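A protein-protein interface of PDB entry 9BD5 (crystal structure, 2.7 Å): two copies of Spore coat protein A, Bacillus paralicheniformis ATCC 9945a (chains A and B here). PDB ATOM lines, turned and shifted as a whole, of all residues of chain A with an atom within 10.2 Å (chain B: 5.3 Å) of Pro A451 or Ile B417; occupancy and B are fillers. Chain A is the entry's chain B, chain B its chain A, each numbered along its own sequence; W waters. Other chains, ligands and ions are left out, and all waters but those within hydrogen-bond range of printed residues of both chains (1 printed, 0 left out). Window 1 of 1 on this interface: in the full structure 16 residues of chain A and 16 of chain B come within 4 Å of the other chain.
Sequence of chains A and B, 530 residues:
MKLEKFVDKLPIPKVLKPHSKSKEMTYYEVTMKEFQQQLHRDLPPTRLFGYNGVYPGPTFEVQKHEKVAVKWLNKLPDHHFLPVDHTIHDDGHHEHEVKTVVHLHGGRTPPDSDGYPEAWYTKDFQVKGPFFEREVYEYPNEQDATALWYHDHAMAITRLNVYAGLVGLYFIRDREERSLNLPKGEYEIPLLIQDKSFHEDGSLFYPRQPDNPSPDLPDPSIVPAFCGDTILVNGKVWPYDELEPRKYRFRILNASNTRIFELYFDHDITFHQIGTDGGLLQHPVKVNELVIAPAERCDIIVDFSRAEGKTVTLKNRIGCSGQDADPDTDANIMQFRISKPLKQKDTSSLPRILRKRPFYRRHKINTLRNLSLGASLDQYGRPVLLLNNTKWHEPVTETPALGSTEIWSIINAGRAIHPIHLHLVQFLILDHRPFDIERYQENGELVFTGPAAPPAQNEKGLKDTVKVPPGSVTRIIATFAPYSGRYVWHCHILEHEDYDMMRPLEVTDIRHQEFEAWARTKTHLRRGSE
Printed residues of chain B within 4 Å of Arg A433: Ile B318 (3.3 Å) and Gly B322 (2.7 Å).
Printed residues of chain B within 4 Å of Phe A448: Gly B322.
Of the printed residues of chain B, Thr A449 touches Gly B322 (3.6 Å).
Of the printed residues of chain A, Val B291 touches Pro A451 (3.8 Å).
Of chain A, only Arg A433, Phe A448, Thr A449 and Gly A450 come within 4 Å of Gly B322.
No residue of chain A comes within 4 Å of Ala B416.
Printed residues of chain A within 4 Å of Ile B417: Pro A451.
His B418 touches none of the printed residues of chain A.
No residue of chain A comes within 4 Å of Pro B469.
The nearest printed residue of chain A that does not touch Val B291 is Ala A452 (4.03 Å).
Among the printed residues, merely in contact across the chains: Arg A433 with Ile B318, Thr A449 with Gly B322, Gly A450 with Ile B318, Pro A451 with Glu B262, Pro A451 with Val B291, Pro A451 with Ile B318 and Pro A451 with Ile B417.
Of the 16 printed residues of chain B, 5 touch a printed residue of chain A.
Hydrophobic or aromatic side chains of chain B that line the printed part of chain A: Val B291, Ile B318 and Ile B417.
Of the 17 printed residues of chain A, 6 touch a printed residue of chain B.
Hydrophobic or aromatic side chains of chain A that line the printed part of chain B: Phe A448, Pro A451 and Ala A452.
Along chain A the printed residues that touch a printed residue of chain B span positions 433 to 452.
Among the printed residues, no Asp or Glu carboxylate lies within 4 Å of a Lys or Arg side-chain nitrogen of the other chain.
Water W1 bridges the backbone carbonyl oxygen of Arg B415 and the backbone carbonyl oxygen of Thr A449.
The backbone carbonyl oxygen of Phe A448 lies close to the backbone carbonyl oxygen of Gly B322 (3.4 Å).
NH2 of Arg A433 is in hydrogen-bond range of O of Gly B322 (2.7 Å).
O of Gly B322 sits close to O of Gly A450.
The side-chain carboxylate of Glu B262 is in hydrogen-bond range of the backbone NH of Ala A452 (3.0 Å).
O of Arg A433 lies within hydrogen-bond range of N of Val A473, 2.7 Å away.
The guanidinium group (NE) of Arg A433 is in hydrogen-bond range of the backbone carbonyl oxygen (O) of Gly A450 (2.9 Å).
N of Thr A449 lies within hydrogen-bond range of O of Pro A434 (3.1 Å).
NZ of Lys B467 is in hydrogen-bond range of O of Val B291.
No position is printed for both chains.
Of the 11 pairs that touch across the chains among the printed residues, none has its exchanged pair printed and touching as well.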
ATOM      1  N   ASP A 431     -29.596   6.666 -14.206  1.00  0.00           N
ATOM      2  CA  ASP A 431     -28.708   7.799 -13.983  1.00  0.00           C
ATOM      3  C   ASP A 431     -27.346   7.295 -13.525  1.00  0.00           C
ATOM      4  O   ASP A 431     -27.176   6.124 -13.174  1.00  0.00           O
ATOM      5  CB  ASP A 431     -29.296   8.777 -12.957  1.00  0.00           C
ATOM      6  CG  ASP A 431     -29.877   8.073 -11.738  1.00  0.00           C
ATOM      7  OD1 ASP A 431     -29.196   7.195 -11.165  1.00  0.00           O
ATOM      8  OD2 ASP A 431     -31.014   8.407 -11.343  1.00  0.00           O
ATOM      9  N   HIS A 432     -26.373   8.205 -13.543  1.00  0.00           N
ATOM     10  CA  HIS A 432     -25.053   7.987 -12.967  1.00  0.00           C
ATOM     11  C   HIS A 432     -24.826   9.006 -11.860  1.00  0.00           C
ATOM     12  O   HIS A 432     -25.338  10.129 -11.917  1.00  0.00           O
ATOM     13  CB  HIS A 432     -23.938   8.118 -14.016  1.00  0.00           C
ATOM     14  CG  HIS A 432     -24.162   7.302 -15.251  1.00  0.00           C
ATOM     15  ND1 HIS A 432     -23.840   5.964 -15.330  1.00  0.00           N
ATOM     16  CD2 HIS A 432     -24.664   7.640 -16.462  1.00  0.00           C
ATOM     17  CE1 HIS A 432     -24.140   5.512 -16.534  1.00  0.00           C
ATOM     18  NE2 HIS A 432     -24.642   6.509 -17.241  1.00  0.00           N
ATOM     19  N   ARG A 433     -24.046   8.617 -10.856  1.00  0.00           N
ATOM     20  CA  ARG A 433     -23.805   9.518  -9.734  1.00  0.00           C
ATOM     21  C   ARG A 433     -22.511   9.163  -9.010  1.00  0.00           C
ATOM     22  O   ARG A 433     -22.286   7.995  -8.670  1.00  0.00           O
ATOM     23  CB  ARG A 433     -24.986   9.480  -8.762  1.00  0.00           C
ATOM     24  CG  ARG A 433     -24.940  10.554  -7.693  1.00  0.00           C
ATOM     25  CD  ARG A 433     -26.175  10.512  -6.819  1.00  0.00           C
ATOM     26  NE  ARG A 433     -26.122  11.522  -5.769  1.00  0.00           N
ATOM     27  CZ  ARG A 433     -26.968  11.586  -4.750  1.00  0.00           C
ATOM     28  NH1 ARG A 433     -27.944  10.705  -4.606  1.00  0.00           N
ATOM     29  NH2 ARG A 433     -26.826  12.555  -3.851  1.00  0.00           N
ATOM     30  N   PRO A 434     -21.644  10.138  -8.754  1.00  0.00           N
ATOM     31  CA  PRO A 434     -20.385   9.848  -8.064  1.00  0.00           C
ATOM     32  C   PRO A 434     -20.599   9.596  -6.579  1.00  0.00           C
ATOM     33  O   PRO A 434     -21.567  10.055  -5.970  1.00  0.00           O
ATOM     34  CB  PRO A 434     -19.563  11.121  -8.288  1.00  0.00           C
ATOM     35  CG  PRO A 434     -20.592  12.196  -8.397  1.00  0.00           C
ATOM     36  CD  PRO A 434     -21.772  11.566  -9.093  1.00  0.00           C
ATOM     37  N   PHE A 435     -19.661   8.851  -5.999  1.00  0.00           N
ATOM     38  CA  PHE A 435     -19.700   8.529  -4.580  1.00  0.00           C
ATOM     39  C   PHE A 435     -18.292   8.611  -4.007  1.00  0.00           C
ATOM     40  O   PHE A 435     -17.308   8.783  -4.730  1.00  0.00           O
ATOM     41  CB  PHE A 435     -20.316   7.144  -4.330  1.00  0.00           C
ATOM     42  CG  PHE A 435     -19.466   5.999  -4.803  1.00  0.00           C
ATOM     43  CD1 PHE A 435     -19.504   5.588  -6.124  1.00  0.00           C
ATOM     44  CD2 PHE A 435     -18.641   5.321  -3.918  1.00  0.00           C
ATOM     45  CE1 PHE A 435     -18.725   4.529  -6.559  1.00  0.00           C
ATOM     46  CE2 PHE A 435     -17.861   4.264  -4.345  1.00  0.00           C
ATOM     47  CZ  PHE A 435     -17.903   3.867  -5.668  1.00  0.00           C
ATOM     48  N   VAL A 447     -21.654   6.794   0.176  1.00  0.00           N
ATOM     49  CA  VAL A 447     -21.890   8.220   0.375  1.00  0.00           C
ATOM     50  C   VAL A 447     -21.680   8.919  -0.959  1.00  0.00           C
ATOM     51  O   VAL A 447     -20.577   8.884  -1.518  1.00  0.00           O
ATOM     52  CB  VAL A 447     -20.966   8.804   1.453  1.00  0.00           C
ATOM     53  CG1 VAL A 447     -21.186  10.305   1.584  1.00  0.00           C
ATOM     54  CG2 VAL A 447     -21.190   8.102   2.783  1.00  0.00           C
ATOM     55  N   PHE A 448     -22.732   9.549  -1.470  1.00  0.00           N
ATOM     56  CA  PHE A 448     -22.633  10.258  -2.736  1.00  0.00           C
ATOM     57  C   PHE A 448     -21.942  11.603  -2.543  1.00  0.00           C
ATOM     58  O   PHE A 448     -22.076  12.253  -1.502  1.00  0.00           O
ATOM     59  CB  PHE A 448     -24.018  10.455  -3.352  1.00  0.00           C
ATOM     60  CG  PHE A 448     -24.700   9.168  -3.720  1.00  0.00           C
ATOM     61  CD1 PHE A 448     -24.259   8.420  -4.799  1.00  0.00           C
ATOM     62  CD2 PHE A 448     -25.779   8.704  -2.985  1.00  0.00           C
ATOM     63  CE1 PHE A 448     -24.883   7.235  -5.142  1.00  0.00           C
ATOM     64  CE2 PHE A 448     -26.407   7.519  -3.322  1.00  0.00           C
ATOM     65  CZ  PHE A 448     -25.958   6.784  -4.402  1.00  0.00           C
ATOM     66  N   THR A 449     -21.183  12.013  -3.561  1.00  0.00           N
ATOM     67  CA  THR A 449     -20.377  13.226  -3.491  1.00  0.00           C
ATOM     68  C   THR A 449     -20.700  14.203  -4.617  1.00  0.00           C
ATOM     69  O   THR A 449     -19.922  15.130  -4.866  1.00  0.00           O
ATOM     70  CB  THR A 449     -18.888  12.880  -3.514  1.00  0.00           C
ATOM     71  OG1 THR A 449     -18.574  12.209  -4.741  1.00  0.00           O
ATOM     72  CG2 THR A 449     -18.531  11.977  -2.341  1.00  0.00           C
ATOM     73  N   GLY A 450     -21.824  14.019  -5.303  1.00  0.00           N
ATOM     74  CA  GLY A 450     -22.183  14.877  -6.406  1.00  0.00           C
ATOM     75  C   GLY A 450     -23.595  14.636  -6.899  1.00  0.00           C
ATOM     76  O   GLY A 450     -24.288  13.718  -6.450  1.00  0.00           O
ATOM     77  N   PRO A 451     -24.048  15.466  -7.834  1.00  0.00           N
ATOM     78  CA  PRO A 451     -25.412  15.318  -8.349  1.00  0.00           C
ATOM     79  C   PRO A 451     -25.526  14.135  -9.298  1.00  0.00           C
ATOM     80  O   PRO A 451     -24.545  13.653  -9.867  1.00  0.00           O
ATOM     81  CB  PRO A 451     -25.656  16.641  -9.080  1.00  0.00           C
ATOM     82  CG  PRO A 451     -24.296  17.061  -9.525  1.00  0.00           C
ATOM     83  CD  PRO A 451     -23.349  16.612  -8.440  1.00  0.00           C
ATOM     84  N   ALA A 452     -26.759  13.662  -9.457  1.00  0.00           N
ATOM     85  CA  ALA A 452     -27.037  12.587 -10.395  1.00  0.00           C
ATOM     86  C   ALA A 452     -27.110  13.132 -11.815  1.00  0.00           C
ATOM     87  O   ALA A 452     -27.508  14.279 -12.045  1.00  0.00           O
ATOM     88  CB  ALA A 452     -28.344  11.878 -10.039  1.00  0.00           C
ATOM     89  N   ALA A 453     -26.716  12.296 -12.772  1.00  0.00           N
ATOM     90  CA  ALA A 453     -26.706  12.677 -14.174  1.00  0.00           C
ATOM     91  C   ALA A 453     -27.410  11.600 -14.988  1.00  0.00           C
ATOM     92  O   ALA A 453     -27.058  10.411 -14.879  1.00  0.00           O
ATOM     93  CB  ALA A 453     -25.275  12.882 -14.684  1.00  0.00           C
ATOM     94  N   PRO A 454     -28.399  11.958 -15.800  1.00  0.00           N
ATOM     95  CA  PRO A 454     -29.037  10.974 -16.674  1.00  0.00           C
ATOM     96  C   PRO A 454     -28.083  10.546 -17.774  1.00  0.00           C
ATOM     97  O   PRO A 454     -27.098  11.247 -18.054  1.00  0.00           O
ATOM     98  CB  PRO A 454     -30.239  11.740 -17.244  1.00  0.00           C
ATOM     99  CG  PRO A 454     -29.799  13.162 -17.229  1.00  0.00           C
ATOM    100  CD  PRO A 454     -28.950  13.310 -15.993  1.00  0.00           C
ATOM    101  N   GLY A 471     -15.630   5.455 -10.172  1.00  0.00           N
ATOM    102  CA  GLY A 471     -16.016   6.280  -9.045  1.00  0.00           C
ATOM    103  C   GLY A 471     -17.459   6.727  -9.057  1.00  0.00           C
ATOM    104  O   GLY A 471     -17.793   7.727  -8.418  1.00  0.00           O
ATOM    105  N   SER A 472     -18.329   6.012  -9.768  1.00  0.00           N
ATOM    106  CA  SER A 472     -19.725   6.395  -9.895  1.00  0.00           C
ATOM    107  C   SER A 472     -20.606   5.169  -9.723  1.00  0.00           C
ATOM    108  O   SER A 472     -20.162   4.029  -9.880  1.00  0.00           O
ATOM    109  CB  SER A 472     -20.010   7.056 -11.250  1.00  0.00           C
ATOM    110  OG  SER A 472     -19.180   8.188 -11.449  1.00  0.00           O
ATOM    111  N   VAL A 473     -21.870   5.420  -9.397  1.00  0.00           N
ATOM    112  CA  VAL A 473     -22.886   4.381  -9.281  1.00  0.00           C
ATOM    113  C   VAL A 473     -23.832   4.524 -10.464  1.00  0.00           C
ATOM    114  O   VAL A 473     -24.479   5.567 -10.626  1.00  0.00           O
ATOM    115  CB  VAL A 473     -23.649   4.474  -7.952  1.00  0.00           C
ATOM    116  CG1 VAL A 473     -24.817   3.500  -7.944  1.00  0.00           C
ATOM    117  CG2 VAL A 473     -22.715   4.197  -6.784  1.00  0.00           C
ATOM    118  N   ARG A 475     -27.211   3.312 -12.057  1.00  0.00           N
ATOM    119  CA  ARG A 475     -28.484   2.667 -11.768  1.00  0.00           C
ATOM    120  C   ARG A 475     -29.127   2.192 -13.065  1.00  0.00           C
ATOM    121  O   ARG A 475     -29.254   2.963 -14.021  1.00  0.00           O
ATOM    122  CB  ARG A 475     -29.419   3.628 -11.034  1.00  0.00           C
ATOM    123  CG  ARG A 475     -29.435   3.458  -9.525  1.00  0.00           C
ATOM    124  CD  ARG A 475     -29.613   4.790  -8.812  1.00  0.00           C
ATOM    125  NE  ARG A 475     -30.665   5.611  -9.401  1.00  0.00           N
ATOM    126  CZ  ARG A 475     -31.943   5.560  -9.052  1.00  0.00           C
ATOM    127  NH1 ARG A 475     -32.376   4.710  -8.134  1.00  0.00           N
ATOM    128  NH2 ARG A 475     -32.809   6.381  -9.637  1.00  0.00           N
ATOM    129  N   ILE B 260     -24.903  23.732  -4.500  1.00  0.00           N
ATOM    130  CA  ILE B 260     -25.405  23.310  -5.804  1.00  0.00           C
ATOM    131  C   ILE B 260     -26.705  22.552  -5.584  1.00  0.00           C
ATOM    132  O   ILE B 260     -26.787  21.687  -4.703  1.00  0.00           O
ATOM    133  CB  ILE B 260     -24.377  22.436  -6.545  1.00  0.00           C
ATOM    134  CG1 ILE B 260     -23.071  23.200  -6.763  1.00  0.00           C
ATOM    135  CG2 ILE B 260     -24.941  21.951  -7.874  1.00  0.00           C
ATOM    136  CD1 ILE B 260     -21.987  22.373  -7.419  1.00  0.00           C
ATOM    137  N   GLU B 262     -30.078  20.216  -7.034  1.00  0.00           N
ATOM    138  CA  GLU B 262     -30.569  19.247  -8.011  1.00  0.00           C
ATOM    139  C   GLU B 262     -32.085  19.221  -7.845  1.00  0.00           C
ATOM    140  O   GLU B 262     -32.626  18.404  -7.095  1.00  0.00           O
ATOM    141  CB  GLU B 262     -29.943  17.872  -7.817  1.00  0.00           C
ATOM    142  CG  GLU B 262     -30.302  16.885  -8.918  1.00  0.00           C
ATOM    143  CD  GLU B 262     -29.536  15.584  -8.811  1.00  0.00           C
ATOM    144  OE1 GLU B 262     -28.628  15.492  -7.962  1.00  0.00           O
ATOM    145  OE2 GLU B 262     -29.843  14.650  -9.577  1.00  0.00           O
ATOM    146  N   VAL B 291     -29.742  20.487 -12.416  1.00  0.00           N
ATOM    147  CA  VAL B 291     -28.543  20.701 -11.614  1.00  0.00           C
ATOM    148  C   VAL B 291     -28.103  22.140 -11.848  1.00  0.00           C
ATOM    149  O   VAL B 291     -27.638  22.488 -12.937  1.00  0.00           O
ATOM    150  CB  VAL B 291     -27.432  19.706 -11.970  1.00  0.00           C
ATOM    151  CG1 VAL B 291     -26.212  19.943 -11.089  1.00  0.00           C
ATOM    152  CG2 VAL B 291     -27.932  18.277 -11.821  1.00  0.00           C
ATOM    153  N   ILE B 318     -29.761  16.665  -3.541  1.00  0.00           N
ATOM    154  CA  ILE B 318     -28.426  16.549  -2.966  1.00  0.00           C
ATOM    155  C   ILE B 318     -28.248  17.555  -1.839  1.00  0.00           C
ATOM    156  O   ILE B 318     -28.867  18.624  -1.816  1.00  0.00           O
ATOM    157  CB  ILE B 318     -27.328  16.735  -4.035  1.00  0.00           C
ATOM    158  CG1 ILE B 318     -27.454  18.106  -4.700  1.00  0.00           C
ATOM    159  CG2 ILE B 318     -27.387  15.618  -5.053  1.00  0.00           C
ATOM    160  CD1 ILE B 318     -26.388  18.393  -5.720  1.00  0.00           C
ATOM    161  N   GLY B 322     -22.880  16.904  -1.982  1.00  0.00           N
ATOM    162  CA  GLY B 322     -23.388  15.956  -2.942  1.00  0.00           C
ATOM    163  C   GLY B 322     -24.085  14.748  -2.357  1.00  0.00           C
ATOM    164  O   GLY B 322     -24.612  13.932  -3.124  1.00  0.00           O
ATOM    165  N   ASN B 412      -9.764  20.772 -13.569  1.00  0.00           N
ATOM    166  CA  ASN B 412     -10.169  20.701 -12.167  1.00  0.00           C
ATOM    167  C   ASN B 412      -9.482  19.503 -11.522  1.00  0.00           C
ATOM    168  O   ASN B 412      -9.909  18.359 -11.697  1.00  0.00           O
ATOM    169  CB  ASN B 412     -11.687  20.605 -12.045  1.00  0.00           C
ATOM    170  CG  ASN B 412     -12.162  20.617 -10.602  1.00  0.00           C
ATOM    171  OD1 ASN B 412     -11.378  20.822  -9.675  1.00  0.00           O
ATOM    172  ND2 ASN B 412     -13.459  20.404 -10.406  1.00  0.00           N
ATOM    173  N   ARG B 415     -11.479  18.090  -5.491  1.00  0.00           N
ATOM    174  CA  ARG B 415     -12.362  17.017  -5.056  1.00  0.00           C
ATOM    175  C   ARG B 415     -13.806  17.225  -5.491  1.00  0.00           C
ATOM    176  O   ARG B 415     -14.545  16.244  -5.640  1.00  0.00           O
ATOM    177  CB  ARG B 415     -12.301  16.878  -3.530  1.00  0.00           C
ATOM    178  CG  ARG B 415     -10.961  17.300  -2.930  1.00  0.00           C
ATOM    179  CD  ARG B 415     -10.640  16.575  -1.624  1.00  0.00           C
ATOM    180  NE  ARG B 415     -11.193  17.226  -0.442  1.00  0.00           N
ATOM    181  CZ  ARG B 415     -10.572  18.166   0.258  1.00  0.00           C
ATOM    182  NH1 ARG B 415      -9.394  18.642  -0.114  1.00  0.00           N
ATOM    183  NH2 ARG B 415     -11.147  18.642   1.360  1.00  0.00           N
ATOM    184  N   ALA B 416     -14.227  18.470  -5.711  1.00  0.00           N
ATOM    185  CA  ALA B 416     -15.626  18.773  -5.972  1.00  0.00           C
ATOM    186  C   ALA B 416     -15.743  19.739  -7.143  1.00  0.00           C
ATOM    187  O   ALA B 416     -14.749  20.241  -7.672  1.00  0.00           O
ATOM    188  CB  ALA B 416     -16.312  19.352  -4.729  1.00  0.00           C
ATOM    189  N   ILE B 417     -16.992  20.000  -7.533  1.00  0.00           N
ATOM    190  CA  ILE B 417     -17.278  20.852  -8.681  1.00  0.00           C
ATOM    191  C   ILE B 417     -16.875  22.290  -8.380  1.00  0.00           C
ATOM    192  O   ILE B 417     -17.003  22.770  -7.247  1.00  0.00           O
ATOM    193  CB  ILE B 417     -18.772  20.758  -9.045  1.00  0.00           C
ATOM    194  CG1 ILE B 417     -19.153  19.316  -9.387  1.00  0.00           C
ATOM    195  CG2 ILE B 417     -19.120  21.684 -10.203  1.00  0.00           C
ATOM    196  CD1 ILE B 417     -20.622  19.136  -9.702  1.00  0.00           C
ATOM    197  N   HIS B 418     -16.373  22.981  -9.401  1.00  0.00           N
ATOM    198  CA  HIS B 418     -16.141  24.419  -9.346  1.00  0.00           C
ATOM    199  C   HIS B 418     -17.004  25.092 -10.404  1.00  0.00           C
ATOM    200  O   HIS B 418     -16.827  24.817 -11.604  1.00  0.00           O
ATOM    201  CB  HIS B 418     -14.665  24.753  -9.574  1.00  0.00           C
ATOM    202  CG  HIS B 418     -13.763  24.322  -8.461  1.00  0.00           C
ATOM    203  ND1 HIS B 418     -13.585  25.069  -7.315  1.00  0.00           N
ATOM    204  CD2 HIS B 418     -12.975  23.231  -8.323  1.00  0.00           C
ATOM    205  CE1 HIS B 418     -12.733  24.451  -6.517  1.00  0.00           C
ATOM    206  NE2 HIS B 418     -12.348  23.333  -7.106  1.00  0.00           N
ATOM    207  N   PRO B 419     -17.952  25.953 -10.030  1.00  0.00           N
ATOM    208  CA  PRO B 419     -18.698  26.713 -11.044  1.00  0.00           C
ATOM    209  C   PRO B 419     -17.918  27.930 -11.519  1.00  0.00           C
ATOM    210  O   PRO B 419     -17.967  28.995 -10.895  1.00  0.00           O
ATOM    211  CB  PRO B 419     -19.981  27.110 -10.306  1.00  0.00           C
ATOM    212  CG  PRO B 419     -19.562  27.203  -8.875  1.00  0.00           C
ATOM    213  CD  PRO B 419     -18.489  26.158  -8.675  1.00  0.00           C
ATOM    214  N   LYS B 467     -20.299  24.284 -14.675  1.00  0.00           N
ATOM    215  CA  LYS B 467     -19.881  23.326 -13.658  1.00  0.00           C
ATOM    216  C   LYS B 467     -18.726  22.500 -14.209  1.00  0.00           C
ATOM    217  O   LYS B 467     -18.901  21.735 -15.163  1.00  0.00           O
ATOM    218  CB  LYS B 467     -21.049  22.430 -13.253  1.00  0.00           C
ATOM    219  CG  LYS B 467     -22.195  23.164 -12.582  1.00  0.00           C
ATOM    220  CD  LYS B 467     -23.318  22.215 -12.200  1.00  0.00           C
ATOM    221  CE  LYS B 467     -24.063  21.711 -13.426  1.00  0.00           C
ATOM    222  NZ  LYS B 467     -24.811  22.802 -14.112  1.00  0.00           N
ATOM    223  N   VAL B 468     -17.545  22.650 -13.616  1.00  0.00           N
ATOM    224  CA  VAL B 468     -16.359  21.902 -14.019  1.00  0.00           C
ATOM    225  C   VAL B 468     -16.247  20.682 -13.106  1.00  0.00           C
ATOM    226  O   VAL B 468     -15.969  20.846 -11.906  1.00  0.00           O
ATOM    227  CB  VAL B 468     -15.095  22.768 -13.953  1.00  0.00           C
ATOM    228  CG1 VAL B 468     -13.892  21.982 -14.443  1.00  0.00           C
ATOM    229  CG2 VAL B 468     -15.279  24.028 -14.783  1.00  0.00           C
ATOM    230  N   PRO B 469     -16.449  19.469 -13.612  1.00  0.00           N
ATOM    231  CA  PRO B 469     -16.486  18.286 -12.743  1.00  0.00           C
ATOM    232  C   PRO B 469     -15.129  18.014 -12.119  1.00  0.00           C
ATOM    233  O   PRO B 469     -14.090  18.429 -12.657  1.00  0.00           O
ATOM    234  CB  PRO B 469     -16.892  17.155 -13.702  1.00  0.00           C
ATOM    235  CG  PRO B 469     -17.490  17.844 -14.890  1.00  0.00           C
ATOM    236  CD  PRO B 469     -16.749  19.135 -15.013  1.00  0.00           C
ATOM    237  N   PRO B 470     -15.095  17.320 -10.983  1.00  0.00           N
ATOM    238  CA  PRO B 470     -13.807  17.001 -10.357  1.00  0.00           C
ATOM    239  C   PRO B 470     -13.061  15.932 -11.141  1.00  0.00           C
ATOM    240  O   PRO B 470     -13.651  14.967 -11.632  1.00  0.00           O
ATOM    241  CB  PRO B 470     -14.206  16.500  -8.964  1.00  0.00           C
ATOM    242  CG  PRO B 470     -15.583  15.962  -9.147  1.00  0.00           C
ATOM    243  CD  PRO B 470     -16.235  16.833 -10.187  1.00  0.00           C
ATOM    244  N   ILE B 493     -18.269  30.197  -6.371  1.00  0.00           N
ATOM    245  CA  ILE B 493     -18.397  29.881  -4.954  1.00  0.00           C
ATOM    246  C   ILE B 493     -17.707  31.009  -4.196  1.00  0.00           C
ATOM    247  O   ILE B 493     -16.478  31.107  -4.196  1.00  0.00           O
ATOM    248  CB  ILE B 493     -17.785  28.519  -4.609  1.00  0.00           C
ATOM    249  CG1 ILE B 493     -18.529  27.400  -5.335  1.00  0.00           C
ATOM    250  CG2 ILE B 493     -17.823  28.288  -3.105  1.00  0.00           C
ATOM    251  CD1 ILE B 493     -17.950  26.024  -5.084  1.00  0.00           C
HETATM  252  O   HOH W   1     -16.899  15.530  -5.413  1.00  0.00           O
